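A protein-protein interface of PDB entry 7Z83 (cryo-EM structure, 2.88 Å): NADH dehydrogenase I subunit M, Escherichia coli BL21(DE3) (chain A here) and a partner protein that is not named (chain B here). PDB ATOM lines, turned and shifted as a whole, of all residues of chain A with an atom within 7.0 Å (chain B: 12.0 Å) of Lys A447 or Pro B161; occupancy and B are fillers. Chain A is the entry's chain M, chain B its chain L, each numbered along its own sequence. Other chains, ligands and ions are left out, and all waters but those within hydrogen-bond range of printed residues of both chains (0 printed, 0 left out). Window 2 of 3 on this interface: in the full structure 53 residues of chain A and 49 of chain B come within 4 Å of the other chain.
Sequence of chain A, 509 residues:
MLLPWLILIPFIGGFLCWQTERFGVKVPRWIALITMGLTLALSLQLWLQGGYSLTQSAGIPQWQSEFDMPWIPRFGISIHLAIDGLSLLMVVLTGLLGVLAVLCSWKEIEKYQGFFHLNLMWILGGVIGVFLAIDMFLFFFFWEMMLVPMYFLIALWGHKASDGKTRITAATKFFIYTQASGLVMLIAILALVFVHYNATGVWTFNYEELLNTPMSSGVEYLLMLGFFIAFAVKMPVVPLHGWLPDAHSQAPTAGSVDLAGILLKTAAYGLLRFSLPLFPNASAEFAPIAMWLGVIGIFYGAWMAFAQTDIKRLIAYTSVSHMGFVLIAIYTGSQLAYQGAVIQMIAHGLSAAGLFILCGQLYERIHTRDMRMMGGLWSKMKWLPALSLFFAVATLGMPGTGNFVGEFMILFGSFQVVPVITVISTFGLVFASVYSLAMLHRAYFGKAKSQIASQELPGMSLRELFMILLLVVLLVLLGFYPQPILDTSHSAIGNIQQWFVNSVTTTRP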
ATOM      1  N   MET A 374      -6.232   1.381   6.050  1.00  0.00           N
ATOM      2  CA  MET A 374      -5.329   0.900   7.083  1.00  0.00           C
ATOM      3  C   MET A 374      -4.744  -0.448   6.690  1.00  0.00           C
ATOM      4  O   MET A 374      -5.301  -1.182   5.872  1.00  0.00           O
ATOM      5  CB  MET A 374      -5.995   0.761   8.462  1.00  0.00           C
ATOM      6  CG  MET A 374      -6.864   1.913   8.906  1.00  0.00           C
ATOM      7  SD  MET A 374      -8.252   1.408   9.957  1.00  0.00           S
ATOM      8  CE  MET A 374      -9.264   0.441   8.866  1.00  0.00           C
ATOM      9  N   GLY A 375      -3.609  -0.765   7.306  1.00  0.00           N
ATOM     10  CA  GLY A 375      -2.926  -2.021   7.080  1.00  0.00           C
ATOM     11  C   GLY A 375      -1.539  -1.993   7.682  1.00  0.00           C
ATOM     12  O   GLY A 375      -0.828  -0.992   7.561  1.00  0.00           O
ATOM     13  N   GLY A 376      -1.142  -3.081   8.333  1.00  0.00           N
ATOM     14  CA  GLY A 376       0.148  -3.113   8.994  1.00  0.00           C
ATOM     15  C   GLY A 376       0.248  -2.225  10.213  1.00  0.00           C
ATOM     16  O   GLY A 376       1.345  -1.774  10.552  1.00  0.00           O
ATOM     17  N   LEU A 377      -0.871  -1.973  10.897  1.00  0.00           N
ATOM     18  CA  LEU A 377      -0.899  -1.076  12.049  1.00  0.00           C
ATOM     19  C   LEU A 377      -0.278  -1.678  13.300  1.00  0.00           C
ATOM     20  O   LEU A 377      -0.182  -0.972  14.310  1.00  0.00           O
ATOM     21  CB  LEU A 377      -2.335  -0.653  12.359  1.00  0.00           C
ATOM     22  CG  LEU A 377      -2.980   0.412  11.475  1.00  0.00           C
ATOM     23  CD1 LEU A 377      -4.453   0.526  11.807  1.00  0.00           C
ATOM     24  CD2 LEU A 377      -2.287   1.749  11.652  1.00  0.00           C
ATOM     25  N   LYS A 380       2.964   0.164  14.386  1.00  0.00           N
ATOM     26  CA  LYS A 380       2.896   1.594  14.655  1.00  0.00           C
ATOM     27  C   LYS A 380       2.218   1.957  15.967  1.00  0.00           C
ATOM     28  O   LYS A 380       2.474   3.048  16.487  1.00  0.00           O
ATOM     29  CB  LYS A 380       2.168   2.315  13.514  1.00  0.00           C
ATOM     30  CG  LYS A 380       2.953   2.358  12.223  1.00  0.00           C
ATOM     31  CD  LYS A 380       2.050   2.715  11.068  1.00  0.00           C
ATOM     32  CE  LYS A 380       1.319   1.487  10.577  1.00  0.00           C
ATOM     33  NZ  LYS A 380       2.256   0.460  10.047  1.00  0.00           N
ATOM     34  N   HIS A 441      -7.082  -8.958   9.543  1.00  0.00           N
ATOM     35  CA  HIS A 441      -6.062  -8.893   8.507  1.00  0.00           C
ATOM     36  C   HIS A 441      -6.251  -7.705   7.572  1.00  0.00           C
ATOM     37  O   HIS A 441      -5.280  -7.261   6.949  1.00  0.00           O
ATOM     38  CB  HIS A 441      -6.023 -10.208   7.733  1.00  0.00           C
ATOM     39  CG  HIS A 441      -5.105 -11.223   8.339  1.00  0.00           C
ATOM     40  ND1 HIS A 441      -3.771 -10.971   8.570  1.00  0.00           N
ATOM     41  CD2 HIS A 441      -5.335 -12.474   8.802  1.00  0.00           C
ATOM     42  CE1 HIS A 441      -3.213 -12.031   9.124  1.00  0.00           C
ATOM     43  NE2 HIS A 441      -4.140 -12.957   9.276  1.00  0.00           N
ATOM     44  N   PHE A 445      -2.887  -5.868   9.820  1.00  0.00           N
ATOM     45  CA  PHE A 445      -1.858  -6.727   9.258  1.00  0.00           C
ATOM     46  C   PHE A 445      -1.686  -6.457   7.770  1.00  0.00           C
ATOM     47  O   PHE A 445      -2.643  -6.124   7.065  1.00  0.00           O
ATOM     48  CB  PHE A 445      -2.194  -8.200   9.486  1.00  0.00           C
ATOM     49  CG  PHE A 445      -2.074  -8.632  10.916  1.00  0.00           C
ATOM     50  CD1 PHE A 445      -1.099  -8.090  11.734  1.00  0.00           C
ATOM     51  CD2 PHE A 445      -2.941  -9.570  11.447  1.00  0.00           C
ATOM     52  CE1 PHE A 445      -0.983  -8.485  13.049  1.00  0.00           C
ATOM     53  CE2 PHE A 445      -2.832  -9.967  12.763  1.00  0.00           C
ATOM     54  CZ  PHE A 445      -1.852  -9.422  13.565  1.00  0.00           C
ATOM     55  N   GLY A 446      -0.451  -6.605   7.300  1.00  0.00           N
ATOM     56  CA  GLY A 446      -0.132  -6.376   5.905  1.00  0.00           C
ATOM     57  C   GLY A 446       0.808  -5.206   5.709  1.00  0.00           C
ATOM     58  O   GLY A 446       1.627  -4.903   6.581  1.00  0.00           O
ATOM     59  N   LYS A 447       0.703  -4.547   4.561  1.00  0.00           N
ATOM     60  CA  LYS A 447       1.450  -3.333   4.275  1.00  0.00           C
ATOM     61  C   LYS A 447       0.482  -2.166   4.136  1.00  0.00           C
ATOM     62  O   LYS A 447      -0.651  -2.332   3.675  1.00  0.00           O
ATOM     63  CB  LYS A 447       2.286  -3.479   3.000  1.00  0.00           C
ATOM     64  CG  LYS A 447       3.695  -4.000   3.237  1.00  0.00           C
ATOM     65  CD  LYS A 447       4.293  -4.585   1.967  1.00  0.00           C
ATOM     66  CE  LYS A 447       3.461  -5.742   1.440  1.00  0.00           C
ATOM     67  NZ  LYS A 447       4.316  -6.873   0.985  1.00  0.00           N
ATOM     68  N   ALA A 448       0.939  -0.988   4.550  1.00  0.00           N
ATOM     69  CA  ALA A 448       0.081   0.190   4.566  1.00  0.00           C
ATOM     70  C   ALA A 448      -0.242   0.644   3.148  1.00  0.00           C
ATOM     71  O   ALA A 448       0.651   0.780   2.308  1.00  0.00           O
ATOM     72  CB  ALA A 448       0.753   1.320   5.340  1.00  0.00           C
ATOM     73  N   LYS A 449      -1.527   0.879   2.885  1.00  0.00           N
ATOM     74  CA  LYS A 449      -1.988   1.382   1.598  1.00  0.00           C
ATOM     75  C   LYS A 449      -2.522   2.807   1.706  1.00  0.00           C
ATOM     76  O   LYS A 449      -3.411   3.204   0.949  1.00  0.00           O
ATOM     77  CB  LYS A 449      -3.046   0.454   1.003  1.00  0.00           C
ATOM     78  CG  LYS A 449      -4.029  -0.117   2.006  1.00  0.00           C
ATOM     79  CD  LYS A 449      -4.242  -1.604   1.764  1.00  0.00           C
ATOM     80  CE  LYS A 449      -5.170  -2.213   2.800  1.00  0.00           C
ATOM     81  NZ  LYS A 449      -5.738  -3.515   2.356  1.00  0.00           N
ATOM     82  N   SER A 450      -1.984   3.586   2.642  1.00  0.00           N
ATOM     83  CA  SER A 450      -2.341   4.988   2.786  1.00  0.00           C
ATOM     84  C   SER A 450      -1.186   5.717   3.457  1.00  0.00           C
ATOM     85  O   SER A 450      -0.293   5.102   4.046  1.00  0.00           O
ATOM     86  CB  SER A 450      -3.635   5.162   3.588  1.00  0.00           C
ATOM     87  OG  SER A 450      -3.425   4.886   4.960  1.00  0.00           O
ATOM     88  N   ALA A 453      -1.516   6.001   7.486  1.00  0.00           N
ATOM     89  CA  ALA A 453      -1.100   4.763   8.125  1.00  0.00           C
ATOM     90  C   ALA A 453       0.361   4.432   7.856  1.00  0.00           C
ATOM     91  O   ALA A 453       0.760   3.273   7.995  1.00  0.00           O
ATOM     92  CB  ALA A 453      -1.993   3.607   7.673  1.00  0.00           C
ATOM     93  N   TYR B 151      -2.622 -20.209  14.322  1.00  0.00           N
ATOM     94  CA  TYR B 151      -2.935 -19.058  13.476  1.00  0.00           C
ATOM     95  C   TYR B 151      -1.976 -17.902  13.730  1.00  0.00           C
ATOM     96  O   TYR B 151      -1.493 -17.267  12.787  1.00  0.00           O
ATOM     97  CB  TYR B 151      -4.379 -18.608  13.712  1.00  0.00           C
ATOM     98  CG  TYR B 151      -4.671 -17.200  13.231  1.00  0.00           C
ATOM     99  CD1 TYR B 151      -4.906 -16.945  11.889  1.00  0.00           C
ATOM    100  CD2 TYR B 151      -4.725 -16.128  14.120  1.00  0.00           C
ATOM    101  CE1 TYR B 151      -5.169 -15.667  11.439  1.00  0.00           C
ATOM    102  CE2 TYR B 151      -4.983 -14.846  13.678  1.00  0.00           C
ATOM    103  CZ  TYR B 151      -5.206 -14.623  12.335  1.00  0.00           C
ATOM    104  OH  TYR B 151      -5.473 -13.352  11.886  1.00  0.00           O
ATOM    105  N   ILE B 154       1.667 -18.969  12.379  1.00  0.00           N
ATOM    106  CA  ILE B 154       1.829 -19.152  10.939  1.00  0.00           C
ATOM    107  C   ILE B 154       1.963 -17.802  10.244  1.00  0.00           C
ATOM    108  O   ILE B 154       2.850 -17.599   9.408  1.00  0.00           O
ATOM    109  CB  ILE B 154       0.662 -19.981  10.374  1.00  0.00           C
ATOM    110  CG1 ILE B 154       0.895 -21.463  10.660  1.00  0.00           C
ATOM    111  CG2 ILE B 154       0.496 -19.756   8.880  1.00  0.00           C
ATOM    112  CD1 ILE B 154      -0.354 -22.299  10.597  1.00  0.00           C
ATOM    113  N   GLY B 155       1.102 -16.852  10.594  1.00  0.00           N
ATOM    114  CA  GLY B 155       1.206 -15.518  10.040  1.00  0.00           C
ATOM    115  C   GLY B 155       2.081 -14.609  10.876  1.00  0.00           C
ATOM    116  O   GLY B 155       1.684 -13.489  11.207  1.00  0.00           O
ATOM    117  N   PHE B 156       3.276 -15.087  11.233  1.00  0.00           N
ATOM    118  CA  PHE B 156       4.162 -14.301  12.083  1.00  0.00           C
ATOM    119  C   PHE B 156       4.750 -13.118  11.327  1.00  0.00           C
ATOM    120  O   PHE B 156       4.796 -12.000  11.851  1.00  0.00           O
ATOM    121  CB  PHE B 156       5.272 -15.183  12.647  1.00  0.00           C
ATOM    122  CG  PHE B 156       6.207 -14.456  13.561  1.00  0.00           C
ATOM    123  CD1 PHE B 156       5.777 -14.009  14.796  1.00  0.00           C
ATOM    124  CD2 PHE B 156       7.516 -14.213  13.183  1.00  0.00           C
ATOM    125  CE1 PHE B 156       6.633 -13.333  15.640  1.00  0.00           C
ATOM    126  CE2 PHE B 156       8.379 -13.539  14.023  1.00  0.00           C
ATOM    127  CZ  PHE B 156       7.936 -13.098  15.252  1.00  0.00           C
ATOM    128  N   TYR B 157       5.208 -13.342  10.094  1.00  0.00           N
ATOM    129  CA  TYR B 157       5.642 -12.251   9.224  1.00  0.00           C
ATOM    130  C   TYR B 157       4.390 -11.644   8.599  1.00  0.00           C
ATOM    131  O   TYR B 157       3.980 -11.978   7.485  1.00  0.00           O
ATOM    132  CB  TYR B 157       6.617 -12.750   8.167  1.00  0.00           C
ATOM    133  CG  TYR B 157       7.788 -13.535   8.709  1.00  0.00           C
ATOM    134  CD1 TYR B 157       8.588 -13.020   9.719  1.00  0.00           C
ATOM    135  CD2 TYR B 157       8.097 -14.791   8.204  1.00  0.00           C
ATOM    136  CE1 TYR B 157       9.662 -13.735  10.213  1.00  0.00           C
ATOM    137  CE2 TYR B 157       9.167 -15.514   8.692  1.00  0.00           C
ATOM    138  CZ  TYR B 157       9.946 -14.981   9.695  1.00  0.00           C
ATOM    139  OH  TYR B 157      11.013 -15.698  10.184  1.00  0.00           O
ATOM    140  N   TYR B 158       3.769 -10.730   9.347  1.00  0.00           N
ATOM    141  CA  TYR B 158       2.475 -10.184   8.958  1.00  0.00           C
ATOM    142  C   TYR B 158       2.561  -9.199   7.802  1.00  0.00           C
ATOM    143  O   TYR B 158       1.517  -8.850   7.242  1.00  0.00           O
ATOM    144  CB  TYR B 158       1.805  -9.508  10.157  1.00  0.00           C
ATOM    145  CG  TYR B 158       2.632  -8.436  10.833  1.00  0.00           C
ATOM    146  CD1 TYR B 158       2.554  -7.109  10.430  1.00  0.00           C
ATOM    147  CD2 TYR B 158       3.475  -8.747  11.890  1.00  0.00           C
ATOM    148  CE1 TYR B 158       3.301  -6.128  11.049  1.00  0.00           C
ATOM    149  CE2 TYR B 158       4.226  -7.772  12.515  1.00  0.00           C
ATOM    150  CZ  TYR B 158       4.136  -6.465  12.091  1.00  0.00           C
ATOM    151  OH  TYR B 158       4.884  -5.495  12.716  1.00  0.00           O
ATOM    152  N   THR B 159       3.762  -8.737   7.444  1.00  0.00           N
ATOM    153  CA  THR B 159       3.900  -7.744   6.383  1.00  0.00           C
ATOM    154  C   THR B 159       3.503  -8.314   5.026  1.00  0.00           C
ATOM    155  O   THR B 159       2.886  -7.616   4.212  1.00  0.00           O
ATOM    156  CB  THR B 159       5.332  -7.217   6.346  1.00  0.00           C
ATOM    157  OG1 THR B 159       6.229  -8.294   6.050  1.00  0.00           O
ATOM    158  CG2 THR B 159       5.705  -6.612   7.687  1.00  0.00           C
ATOM    159  N   ASP B 160       3.847  -9.567   4.763  1.00  0.00           N
ATOM    160  CA  ASP B 160       3.455 -10.215   3.517  1.00  0.00           C
ATOM    161  C   ASP B 160       2.001 -10.663   3.613  1.00  0.00           C
ATOM    162  O   ASP B 160       1.659 -11.421   4.528  1.00  0.00           O
ATOM    163  CB  ASP B 160       4.360 -11.408   3.238  1.00  0.00           C
ATOM    164  CG  ASP B 160       4.174 -11.981   1.844  1.00  0.00           C
ATOM    165  OD1 ASP B 160       3.541 -11.322   0.995  1.00  0.00           O
ATOM    166  OD2 ASP B 160       4.668 -13.101   1.595  1.00  0.00           O
ATOM    167  N   PRO B 161       1.117 -10.208   2.717  1.00  0.00           N
ATOM    168  CA  PRO B 161      -0.285 -10.660   2.770  1.00  0.00           C
ATOM    169  C   PRO B 161      -0.475 -12.141   2.482  1.00  0.00           C
ATOM    170  O   PRO B 161      -1.516 -12.695   2.863  1.00  0.00           O
ATOM    171  CB  PRO B 161      -0.973  -9.797   1.703  1.00  0.00           C
ATOM    172  CG  PRO B 161      -0.092  -8.602   1.557  1.00  0.00           C
ATOM    173  CD  PRO B 161       1.303  -9.109   1.755  1.00  0.00           C
ATOM    174  N   LYS B 162       0.484 -12.795   1.820  1.00  0.00           N
ATOM    175  CA  LYS B 162       0.363 -14.227   1.565  1.00  0.00           C
ATOM    176  C   LYS B 162       0.432 -15.025   2.861  1.00  0.00           C
ATOM    177  O   LYS B 162      -0.254 -16.045   3.005  1.00  0.00           O
ATOM    178  CB  LYS B 162       1.452 -14.680   0.592  1.00  0.00           C
ATOM    179  CG  LYS B 162       1.494 -13.891  -0.710  1.00  0.00           C
ATOM    180  CD  LYS B 162       1.194 -14.767  -1.923  1.00  0.00           C
ATOM    181  CE  LYS B 162      -0.213 -15.346  -1.879  1.00  0.00           C
ATOM    182  NZ  LYS B 162      -0.654 -15.831  -3.215  1.00  0.00           N
ATOM    183  N   ASN B 163       1.244 -14.567   3.817  1.00  0.00           N
ATOM    184  CA  ASN B 163       1.283 -15.204   5.129  1.00  0.00           C
ATOM    185  C   ASN B 163      -0.053 -15.057   5.847  1.00  0.00           C
ATOM    186  O   ASN B 163      -0.521 -15.993   6.508  1.00  0.00           O
ATOM    187  CB  ASN B 163       2.408 -14.605   5.970  1.00  0.00           C
ATOM    188  CG  ASN B 163       3.739 -14.608   5.251  1.00  0.00           C
ATOM    189  OD1 ASN B 163       3.970 -15.410   4.348  1.00  0.00           O
ATOM    190  ND2 ASN B 163       4.629 -13.717   5.660  1.00  0.00           N
ATOM    191  N   GLY B 164      -0.682 -13.887   5.717  1.00  0.00           N
ATOM    192  CA  GLY B 164      -1.995 -13.692   6.306  1.00  0.00           C
ATOM    193  C   GLY B 164      -3.060 -14.563   5.670  1.00  0.00           C
ATOM    194  O   GLY B 164      -3.937 -15.086   6.361  1.00  0.00           O
ATOM    195  N   ALA B 165      -2.998 -14.737   4.347  1.00  0.00           N
ATOM    196  CA  ALA B 165      -3.946 -15.621   3.673  1.00  0.00           C
ATOM    197  C   ALA B 165      -3.730 -17.076   4.077  1.00  0.00           C
ATOM    198  O   ALA B 165      -4.696 -17.837   4.228  1.00  0.00           O
ATOM    199  CB  ALA B 165      -3.833 -15.460   2.159  1.00  0.00           C
ATOM    200  N   ALA B 166      -2.468 -17.475   4.255  1.00  0.00           N
ATOM    201  CA  ALA B 166      -2.165 -18.819   4.736  1.00  0.00           C
ATOM    202  C   ALA B 166      -2.712 -19.043   6.140  1.00  0.00           C
ATOM    203  O   ALA B 166      -3.290 -20.100   6.430  1.00  0.00           O
ATOM    204  CB  ALA B 166      -0.656 -19.046   4.712  1.00  0.00           C
ATOM    205  N   ALA B 167      -2.540 -18.054   7.020  1.00  0.00           N
ATOM    206  CA  ALA B 167      -3.078 -18.150   8.374  1.00  0.00           C
ATOM    207  C   ALA B 167      -4.603 -18.191   8.362  1.00  0.00           C
ATOM    208  O   ALA B 167      -5.216 -18.922   9.152  1.00  0.00           O
ATOM    209  CB  ALA B 167      -2.569 -16.979   9.214  1.00  0.00           C
ATOM    210  N   MET B 168      -5.226 -17.415   7.466  1.00  0.00           N
ATOM    211  CA  MET B 168      -6.672 -17.471   7.267  1.00  0.00           C
ATOM    212  C   MET B 168      -7.132 -18.873   6.898  1.00  0.00           C
ATOM    213  O   MET B 168      -8.059 -19.413   7.511  1.00  0.00           O
ATOM    214  CB  MET B 168      -7.092 -16.494   6.168  1.00  0.00           C
ATOM    215  CG  MET B 168      -8.288 -15.615   6.493  1.00  0.00           C
ATOM    216  SD  MET B 168      -7.851 -14.017   7.180  1.00  0.00           S
ATOM    217  CE  MET B 168      -7.259 -13.167   5.719  1.00  0.00           C
ATOM    218  N   LYS B 169      -6.498 -19.473   5.886  1.00  0.00           N
ATOM    219  CA  LYS B 169      -6.913 -20.796   5.425  1.00  0.00           C
ATOM    220  C   LYS B 169      -6.701 -21.849   6.505  1.00  0.00           C
ATOM    221  O   LYS B 169      -7.558 -22.723   6.709  1.00  0.00           O
ATOM    222  CB  LYS B 169      -6.155 -21.166   4.150  1.00  0.00           C
ATOM    223  CG  LYS B 169      -6.700 -22.385   3.431  1.00  0.00           C
ATOM    224  CD  LYS B 169      -5.586 -23.161   2.751  1.00  0.00           C
ATOM    225  CE  LYS B 169      -5.969 -23.546   1.332  1.00  0.00           C
ATOM    226  NZ  LYS B 169      -7.364 -24.058   1.251  1.00  0.00           N
ATOM    227  N   ALA B 170      -5.578 -21.757   7.227  1.00  0.00           N
ATOM    228  CA  ALA B 170      -5.297 -22.687   8.317  1.00  0.00           C
ATOM    229  C   ALA B 170      -6.357 -22.601   9.406  1.00  0.00           C
ATOM    230  O   ALA B 170      -6.913 -23.623   9.830  1.00  0.00           O
ATOM    231  CB  ALA B 170      -3.914 -22.403   8.897  1.00  0.00           C
ATOM    232  N   ASP B 241       0.206 -24.647   2.415  1.00  0.00           N
ATOM    233  CA  ASP B 241       0.060 -23.204   2.278  1.00  0.00           C
ATOM    234  C   ASP B 241       0.456 -22.484   3.561  1.00  0.00           C
ATOM    235  O   ASP B 241       1.128 -21.448   3.512  1.00  0.00           O
ATOM    236  CB  ASP B 241      -1.375 -22.862   1.882  1.00  0.00           C
ATOM    237  CG  ASP B 241      -1.938 -23.822   0.851  1.00  0.00           C
ATOM    238  OD1 ASP B 241      -1.598 -25.022   0.905  1.00  0.00           O
ATOM    239  OD2 ASP B 241      -2.721 -23.375  -0.013  1.00  0.00           O
ATOM    240  N   ALA B 242       0.096 -23.041   4.718  1.00  0.00           N
ATOM    241  CA  ALA B 242       0.333 -22.431   6.017  1.00  0.00           C
ATOM    242  C   ALA B 242       1.733 -22.693   6.547  1.00  0.00           C
ATOM    243  O   ALA B 242       1.983 -22.501   7.739  1.00  0.00           O
ATOM    244  CB  ALA B 242      -0.707 -22.929   7.019  1.00  0.00           C
ATOM    245  N   MET B 243       2.627 -23.152   5.700  1.00  0.00           N
ATOM    246  CA  MET B 243       4.078 -23.107   5.958  1.00  0.00           C
ATOM    247  C   MET B 243       4.637 -21.680   6.287  1.00  0.00           C
ATOM    248  O   MET B 243       5.806 -21.607   6.689  1.00  0.00           O
ATOM    249  CB  MET B 243       4.826 -23.599   4.725  1.00  0.00           C
ATOM    250  CG  MET B 243       6.148 -24.261   4.996  1.00  0.00           C
ATOM    251  SD  MET B 243       5.739 -25.870   5.624  1.00  0.00           S
ATOM    252  CE  MET B 243       4.998 -26.421   4.104  1.00  0.00           C
ATOM    253  N   ALA B 244       3.872 -20.589   6.178  1.00  0.00           N
ATOM    254  CA  ALA B 244       4.401 -19.234   6.069  1.00  0.00           C
ATOM    255  C   ALA B 244       5.139 -18.746   7.308  1.00  0.00           C
ATOM    256  O   ALA B 244       5.835 -17.728   7.225  1.00  0.00           O
ATOM    257  CB  ALA B 244       3.262 -18.272   5.744  1.00  0.00           C
ATOM    258  N   GLY B 245       5.016 -19.430   8.442  1.00  0.00           N
ATOM    259  CA  GLY B 245       5.750 -19.044   9.620  1.00  0.00           C
ATOM    260  C   GLY B 245       7.201 -19.459   9.545  1.00  0.00           C
ATOM    261  O   GLY B 245       7.659 -20.091   8.585  1.00  0.00           O
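OH of Tyr B151 lies within hydrogen-bond range of NE2 of His A441 (3.0 Å).
The backbone NH (N) of Gly A446 sits at hydrogen-bond distance from the backbone carbonyl oxygen (O) of Tyr B158 (3.0 Å).
Among the printed residues, pairs that only touch across the chains: His A441 with Gly B164 (3.5 Å), His A441 with Met B168 (3.4 Å), Phe A445 with Tyr B158 (3.6 Å), Gly A446 with Thr B159 (3.5 Å), Lys A447 with Thr B159 (3.4 Å) and Lys A447 with Pro B161 (3.8 Å).
Of the printed residues of chain B, Lys A447 touches Thr B159 (3.4 Å) and Pro B161 (3.8 Å).
Of chain A, only Lys A447 comes within 4 Å of Pro B161.
No residue of chain B comes within 4 Å of Gly A376.
Gly A446 touches just these residues of chain B: Tyr B158 and Thr B159.
Ala A448 touches none of the printed residues of chain B.
No residue of chain B comes within 4 Å of Lys A449.
Printed residues of chain A within 4 Å of Tyr B151: His A441 (3.0 Å).
Printed residues of chain B within 4 Å of His A441: Tyr B151, Gly B164 and Met B168.
Ser A450 touches none of the printed residues of chain B.
Tyr B157 touches none of the printed residues of chain A.
The nearest residue of chain B that does not touch Lys A447 is Asp B160 (4.3 Å).
The nearest printed residue of chain A that does not touch Tyr B158 is Gly A376 (4.8 Å).
Hydrophobic or aromatic side chains of chain A within 4 Å of the printed part of chain B: His A441 and Phe A445.
Of the 23 printed residues of chain B, 6 touch a printed residue of chain A.
Among the printed residues, no Asp or Glu carboxylate lies within 4 Å of a Lys or Arg side-chain nitrogen of the other chain.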
